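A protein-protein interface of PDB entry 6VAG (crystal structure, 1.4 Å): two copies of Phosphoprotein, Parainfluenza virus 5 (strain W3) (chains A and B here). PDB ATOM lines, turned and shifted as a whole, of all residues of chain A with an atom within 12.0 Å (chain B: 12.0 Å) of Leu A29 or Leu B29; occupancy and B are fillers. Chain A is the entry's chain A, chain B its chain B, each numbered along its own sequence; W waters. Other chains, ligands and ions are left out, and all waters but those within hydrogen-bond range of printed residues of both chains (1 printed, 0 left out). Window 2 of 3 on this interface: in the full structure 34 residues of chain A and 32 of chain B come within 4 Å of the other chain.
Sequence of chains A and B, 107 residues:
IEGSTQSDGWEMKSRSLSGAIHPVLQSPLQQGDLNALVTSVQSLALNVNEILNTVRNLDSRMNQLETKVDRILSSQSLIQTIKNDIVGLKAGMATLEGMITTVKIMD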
ATOM      1  N   SER A  27      34.198  -6.138  -2.705  1.00  0.00           N
ATOM      2  CA  SER A  27      32.884  -5.709  -3.160  1.00  0.00           C
ATOM      3  C   SER A  27      32.358  -6.687  -4.194  1.00  0.00           C
ATOM      4  O   SER A  27      33.045  -6.992  -5.162  1.00  0.00           O
ATOM      5  CB  SER A  27      32.959  -4.311  -3.772  1.00  0.00           C
ATOM      6  OG  SER A  27      31.740  -3.610  -3.592  1.00  0.00           O
ATOM      7  N   PRO A  28      31.139  -7.179  -3.994  1.00  0.00           N
ATOM      8  CA  PRO A  28      30.552  -8.103  -4.974  1.00  0.00           C
ATOM      9  C   PRO A  28      30.424  -7.447  -6.340  1.00  0.00           C
ATOM     10  O   PRO A  28      30.077  -6.269  -6.454  1.00  0.00           O
ATOM     11  CB  PRO A  28      29.172  -8.416  -4.387  1.00  0.00           C
ATOM     12  CG  PRO A  28      29.232  -7.984  -2.953  1.00  0.00           C
ATOM     13  CD  PRO A  28      30.229  -6.885  -2.872  1.00  0.00           C
ATOM     14  N   LEU A  29      30.706  -8.233  -7.379  1.00  0.00           N
ATOM     15  CA  LEU A  29      30.491  -7.782  -8.751  1.00  0.00           C
ATOM     16  C   LEU A  29      29.002  -7.524  -8.971  1.00  0.00           C
ATOM     17  O   LEU A  29      28.153  -8.315  -8.549  1.00  0.00           O
ATOM     18  CB  LEU A  29      30.983  -8.861  -9.721  1.00  0.00           C
ATOM     19  CG  LEU A  29      31.099  -8.467 -11.200  1.00  0.00           C
ATOM     20  CD1 LEU A  29      32.102  -7.335 -11.414  1.00  0.00           C
ATOM     21  CD2 LEU A  29      31.488  -9.676 -12.031  1.00  0.00           C
ATOM     22  N   GLN A  30      28.684  -6.407  -9.633  1.00  0.00           N
ATOM     23  CA  GLN A  30      27.307  -6.002  -9.868  1.00  0.00           C
ATOM     24  C   GLN A  30      27.057  -5.833 -11.363  1.00  0.00           C
ATOM     25  O   GLN A  30      27.990  -5.684 -12.161  1.00  0.00           O
ATOM     26  CB  GLN A  30      27.003  -4.668  -9.168  1.00  0.00           C
ATOM     27  CG  GLN A  30      27.331  -4.644  -7.693  1.00  0.00           C
ATOM     28  CD  GLN A  30      26.252  -5.294  -6.873  1.00  0.00           C
ATOM     29  OE1 GLN A  30      25.069  -5.157  -7.177  1.00  0.00           O
ATOM     30  NE2 GLN A  30      26.646  -6.000  -5.817  1.00  0.00           N
ATOM     31  N   GLN A  31      25.777  -5.851 -11.748  1.00  0.00           N
ATOM     32  CA  GLN A  31      25.433  -5.627 -13.153  1.00  0.00           C
ATOM     33  C   GLN A  31      26.013  -4.313 -13.671  1.00  0.00           C
ATOM     34  O   GLN A  31      26.487  -4.244 -14.813  1.00  0.00           O
ATOM     35  CB  GLN A  31      23.915  -5.648 -13.348  1.00  0.00           C
ATOM     36  CG  GLN A  31      23.485  -5.524 -14.807  1.00  0.00           C
ATOM     37  CD  GLN A  31      23.817  -6.770 -15.595  1.00  0.00           C
ATOM     38  OE1 GLN A  31      23.526  -7.882 -15.161  1.00  0.00           O
ATOM     39  NE2 GLN A  31      24.430  -6.598 -16.763  1.00  0.00           N
ATOM     40  N   GLY A  32      26.017  -3.269 -12.837  1.00  0.00           N
ATOM     41  CA  GLY A  32      26.560  -1.989 -13.264  1.00  0.00           C
ATOM     42  C   GLY A  32      28.022  -2.064 -13.663  1.00  0.00           C
ATOM     43  O   GLY A  32      28.468  -1.312 -14.538  1.00  0.00           O
ATOM     44  N   ASP A  33      28.784  -2.980 -13.054  1.00  0.00           N
ATOM     45  CA  ASP A  33      30.182  -3.182 -13.449  1.00  0.00           C
ATOM     46  C   ASP A  33      30.296  -3.742 -14.865  1.00  0.00           C
ATOM     47  O   ASP A  33      31.184  -3.342 -15.640  1.00  0.00           O
ATOM     48  CB  ASP A  33      30.855  -4.145 -12.463  1.00  0.00           C
ATOM     49  CG  ASP A  33      30.922  -3.584 -11.057  1.00  0.00           C
ATOM     50  OD1 ASP A  33      31.429  -2.458 -10.896  1.00  0.00           O
ATOM     51  OD2 ASP A  33      30.475  -4.258 -10.113  1.00  0.00           O
ATOM     52  N   LEU A  34      29.425  -4.690 -15.221  1.00  0.00           N
ATOM     53  CA  LEU A  34      29.407  -5.202 -16.586  1.00  0.00           C
ATOM     54  C   LEU A  34      28.926  -4.128 -17.550  1.00  0.00           C
ATOM     55  O   LEU A  34      29.479  -3.972 -18.652  1.00  0.00           O
ATOM     56  CB  LEU A  34      28.482  -6.414 -16.669  1.00  0.00           C
ATOM     57  CG  LEU A  34      28.824  -7.553 -15.710  1.00  0.00           C
ATOM     58  CD1 LEU A  34      27.871  -8.723 -15.925  1.00  0.00           C
ATOM     59  CD2 LEU A  34      30.282  -8.003 -15.838  1.00  0.00           C
ATOM     60  N   ASN A  35      27.896  -3.378 -17.151  1.00  0.00           N
ATOM     61  CA  ASN A  35      27.349  -2.339 -18.012  1.00  0.00           C
ATOM     62  C   ASN A  35      28.385  -1.263 -18.312  1.00  0.00           C
ATOM     63  O   ASN A  35      28.413  -0.710 -19.422  1.00  0.00           O
ATOM     64  CB  ASN A  35      26.122  -1.693 -17.358  1.00  0.00           C
ATOM     65  CG  ASN A  35      24.958  -2.655 -17.195  1.00  0.00           C
ATOM     66  OD1 ASN A  35      24.966  -3.777 -17.720  1.00  0.00           O
ATOM     67  ND2 ASN A  35      23.940  -2.221 -16.451  1.00  0.00           N
ATOM     68  N   ALA A  36      29.248  -0.958 -17.343  1.00  0.00           N
ATOM     69  CA  ALA A  36      30.319   0.011 -17.565  1.00  0.00           C
ATOM     70  C   ALA A  36      31.242  -0.438 -18.692  1.00  0.00           C
ATOM     71  O   ALA A  36      31.637   0.372 -19.549  1.00  0.00           O
ATOM     72  CB  ALA A  36      31.109   0.195 -16.271  1.00  0.00           C
ATOM     73  N   LEU A  37      31.576  -1.733 -18.728  1.00  0.00           N
ATOM     74  CA  LEU A  37      32.410  -2.259 -19.810  1.00  0.00           C
ATOM     75  C   LEU A  37      31.681  -2.219 -21.149  1.00  0.00           C
ATOM     76  O   LEU A  37      32.292  -1.914 -22.182  1.00  0.00           O
ATOM     77  CB  LEU A  37      32.869  -3.674 -19.482  1.00  0.00           C
ATOM     78  CG  LEU A  37      34.102  -3.736 -18.591  1.00  0.00           C
ATOM     79  CD1 LEU A  37      34.418  -5.181 -18.238  1.00  0.00           C
ATOM     80  CD2 LEU A  37      35.292  -3.062 -19.271  1.00  0.00           C
ATOM     81  N   VAL A  38      30.378  -2.516 -21.168  1.00  0.00           N
ATOM     82  CA  VAL A  38      29.620  -2.402 -22.412  1.00  0.00           C
ATOM     83  C   VAL A  38      29.740  -0.996 -22.991  1.00  0.00           C
ATOM     84  O   VAL A  38      30.050  -0.817 -24.179  1.00  0.00           O
ATOM     85  CB  VAL A  38      28.144  -2.783 -22.195  1.00  0.00           C
ATOM     86  CG1 VAL A  38      27.334  -2.536 -23.482  1.00  0.00           C
ATOM     87  CG2 VAL A  38      28.018  -4.246 -21.761  1.00  0.00           C
ATOM     88  N   PRO B  28      22.586 -12.901  -7.527  1.00  0.00           N
ATOM     89  CA  PRO B  28      23.675 -13.602  -8.216  1.00  0.00           C
ATOM     90  C   PRO B  28      23.637 -13.396  -9.725  1.00  0.00           C
ATOM     91  O   PRO B  28      22.668 -13.748 -10.392  1.00  0.00           O
ATOM     92  CB  PRO B  28      23.402 -15.067  -7.885  1.00  0.00           C
ATOM     93  CG  PRO B  28      21.925 -15.135  -7.736  1.00  0.00           C
ATOM     94  CD  PRO B  28      21.481 -13.809  -7.172  1.00  0.00           C
ATOM     95  N   LEU B  29      24.707 -12.825 -10.258  1.00  0.00           N
ATOM     96  CA  LEU B  29      24.777 -12.605 -11.694  1.00  0.00           C
ATOM     97  C   LEU B  29      24.664 -13.934 -12.431  1.00  0.00           C
ATOM     98  O   LEU B  29      25.168 -14.964 -11.970  1.00  0.00           O
ATOM     99  CB  LEU B  29      26.097 -11.919 -12.042  1.00  0.00           C
ATOM    100  CG  LEU B  29      26.216 -10.468 -11.570  1.00  0.00           C
ATOM    101  CD1 LEU B  29      27.632  -9.953 -11.767  1.00  0.00           C
ATOM    102  CD2 LEU B  29      25.200  -9.574 -12.288  1.00  0.00           C
ATOM    103  N   GLN B  30      24.011 -13.898 -13.591  1.00  0.00           N
ATOM    104  CA  GLN B  30      23.775 -15.051 -14.443  1.00  0.00           C
ATOM    105  C   GLN B  30      24.585 -14.908 -15.727  1.00  0.00           C
ATOM    106  O   GLN B  30      25.009 -13.812 -16.096  1.00  0.00           O
ATOM    107  CB  GLN B  30      22.286 -15.148 -14.793  1.00  0.00           C
ATOM    108  CG  GLN B  30      21.382 -15.286 -13.580  1.00  0.00           C
ATOM    109  CD  GLN B  30      21.628 -16.576 -12.839  1.00  0.00           C
ATOM    110  OE1 GLN B  30      21.971 -16.572 -11.655  1.00  0.00           O
ATOM    111  NE2 GLN B  30      21.458 -17.696 -13.534  1.00  0.00           N
ATOM    112  N   GLN B  31      24.794 -16.032 -16.419  1.00  0.00           N
ATOM    113  CA  GLN B  31      25.518 -15.987 -17.688  1.00  0.00           C
ATOM    114  C   GLN B  31      24.909 -14.964 -18.634  1.00  0.00           C
ATOM    115  O   GLN B  31      25.633 -14.234 -19.326  1.00  0.00           O
ATOM    116  CB  GLN B  31      25.506 -17.370 -18.333  1.00  0.00           C
ATOM    117  CG  GLN B  31      26.661 -18.254 -17.906  1.00  0.00           C
ATOM    118  CD  GLN B  31      26.712 -19.550 -18.685  1.00  0.00           C
ATOM    119  OE1 GLN B  31      25.770 -20.341 -18.657  1.00  0.00           O
ATOM    120  NE2 GLN B  31      27.811 -19.769 -19.396  1.00  0.00           N
ATOM    121  N   GLY B  32      23.576 -14.909 -18.699  1.00  0.00           N
ATOM    122  CA  GLY B  32      22.913 -13.988 -19.606  1.00  0.00           C
ATOM    123  C   GLY B  32      23.178 -12.529 -19.306  1.00  0.00           C
ATOM    124  O   GLY B  32      23.002 -11.681 -20.193  1.00  0.00           O
ATOM    125  N   ASP B  33      23.609 -12.213 -18.082  1.00  0.00           N
ATOM    126  CA  ASP B  33      23.956 -10.836 -17.751  1.00  0.00           C
ATOM    127  C   ASP B  33      25.185 -10.343 -18.510  1.00  0.00           C
ATOM    128  O   ASP B  33      25.406  -9.133 -18.587  1.00  0.00           O
ATOM    129  CB  ASP B  33      24.127 -10.696 -16.234  1.00  0.00           C
ATOM    130  CG  ASP B  33      22.825 -10.929 -15.497  1.00  0.00           C
ATOM    131  OD1 ASP B  33      21.768 -10.497 -16.012  1.00  0.00           O
ATOM    132  OD2 ASP B  33      22.842 -11.556 -14.425  1.00  0.00           O
ATOM    133  N   LEU B  34      25.969 -11.254 -19.078  1.00  0.00           N
ATOM    134  CA  LEU B  34      27.147 -10.913 -19.862  1.00  0.00           C
ATOM    135  C   LEU B  34      26.843 -10.775 -21.352  1.00  0.00           C
ATOM    136  O   LEU B  34      27.733 -10.385 -22.120  1.00  0.00           O
ATOM    137  CB  LEU B  34      28.219 -11.990 -19.654  1.00  0.00           C
ATOM    138  CG  LEU B  34      29.675 -11.566 -19.848  1.00  0.00           C
ATOM    139  CD1 LEU B  34      30.056 -10.494 -18.828  1.00  0.00           C
ATOM    140  CD2 LEU B  34      30.590 -12.776 -19.735  1.00  0.00           C
ATOM    141  N   ASN B  35      25.618 -11.082 -21.786  1.00  0.00           N
ATOM    142  CA  ASN B  35      25.335 -11.145 -23.218  1.00  0.00           C
ATOM    143  C   ASN B  35      25.638  -9.828 -23.924  1.00  0.00           C
ATOM    144  O   ASN B  35      26.214  -9.826 -25.019  1.00  0.00           O
ATOM    145  CB  ASN B  35      23.875 -11.501 -23.454  1.00  0.00           C
ATOM    146  CG  ASN B  35      23.592 -12.958 -23.224  1.00  0.00           C
ATOM    147  OD1 ASN B  35      24.487 -13.774 -22.962  1.00  0.00           O
ATOM    148  ND2 ASN B  35      22.333 -13.292 -23.311  1.00  0.00           N
ATOM    149  N   ALA B  36      25.237  -8.694 -23.339  1.00  0.00           N
ATOM    150  CA  ALA B  36      25.450  -7.426 -24.034  1.00  0.00           C
ATOM    151  C   ALA B  36      26.931  -7.176 -24.257  1.00  0.00           C
ATOM    152  O   ALA B  36      27.331  -6.686 -25.322  1.00  0.00           O
ATOM    153  CB  ALA B  36      24.815  -6.266 -23.270  1.00  0.00           C
ATOM    154  N   LEU B  37      27.765  -7.509 -23.268  1.00  0.00           N
ATOM    155  CA  LEU B  37      29.202  -7.333 -23.423  1.00  0.00           C
ATOM    156  C   LEU B  37      29.763  -8.270 -24.486  1.00  0.00           C
ATOM    157  O   LEU B  37      30.576  -7.852 -25.319  1.00  0.00           O
ATOM    158  CB  LEU B  37      29.897  -7.542 -22.079  1.00  0.00           C
ATOM    159  CG  LEU B  37      31.370  -7.138 -22.023  1.00  0.00           C
ATOM    160  CD1 LEU B  37      31.629  -5.748 -22.631  1.00  0.00           C
ATOM    161  CD2 LEU B  37      31.892  -7.220 -20.591  1.00  0.00           C
HETATM  162  O   HOH W   1      21.200  -8.276 -17.685  1.00  0.00           O
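Of the printed residues of chain B, Leu A29 touches Leu B29. Gln A31 touches just these residues of chain B: Leu B29 and Asp B33. No residue of chain B comes within 4 Å of Gly A32. No residue of chain A comes within 4 Å of Gln B30. Asp B33 touches just these residues of chain A: Gln A31 and Leu A34. Of the printed residues of chain B, Leu A37 touches Leu B37. Printed residues of chain A within 4 Å of Leu B34: Leu A34. Gln B31 touches none of the printed residues of chain A. Asn A35 touches none of the printed residues of chain B. The nearest residue of chain B that does not touch Leu A29 is Pro B28 (6.9 Å).
Among the printed residues, merely in contact across the chains: Val A38 with Leu B37 (3.6 Å), Leu A29 with Leu B29 (3.6 Å), Leu A34 with Asp B33 (3.7 Å), Gln A31 with Leu B29 (3.7 Å), Leu A37 with Leu B37 (3.8 Å), Leu A34 with Leu B34 (3.9 Å) and Val A38 with Ala B36 (3.9996 Å).
Water W1 bridges OD1 of Asp B33 (2.8 Å) and OE1 of Gln A31 (3.5 Å).
Leu B29 touches its own counterpart, Leu A29. Gln A31 touches Leu B29, but with the chains exchanged Leu A29 does not touch Gln B31 (10.2 Å). Gln A31 touches Asp B33, but with the chains exchanged Asp A33 does not touch Gln B31 (12.3 Å). Leu A34 touches its own counterpart, Leu B34. 10 positions are printed for both chains. Of the 8 pairs that touch across the chains among the printed residues, 3 have their exchanged pair printed and touching as well.
Printed residues of chain A that touch a printed residue of chain B: Leu A29, Gln A31, Leu A34, Leu A37 and Val A38. Printed residues of chain B that touch a printed residue of chain A: Leu B29, Asp B33, Leu B34, Ala B36 and Leu B37. Hydrophobic or aromatic side chains of chain B within 4 Å of the printed part of chain A: Leu B29, Leu B34 and Leu B37. Among the printed residues, 8 pairs touch across the chains. Among the printed residues, no Asp or Glu carboxylate lies within 4 Å of a Lys or Arg side-chain nitrogen of the other chain.
The side-chain carboxylate (OD1) of Asp B33 sits close to the side-chain amide oxygen (OE1) of Gln A31 (3.3 Å).
The side-chain carboxylate (OD2) of Asp B33 sits at hydrogen-bond distance from the backbone NH (N) of Gln B30, 2.7 Å away. The side-chain amide nitrogen (NE2) of Gln A31 sits at hydrogen-bond distance from the side-chain amide oxygen (OD1) of Asn A35 (3.0 Å).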
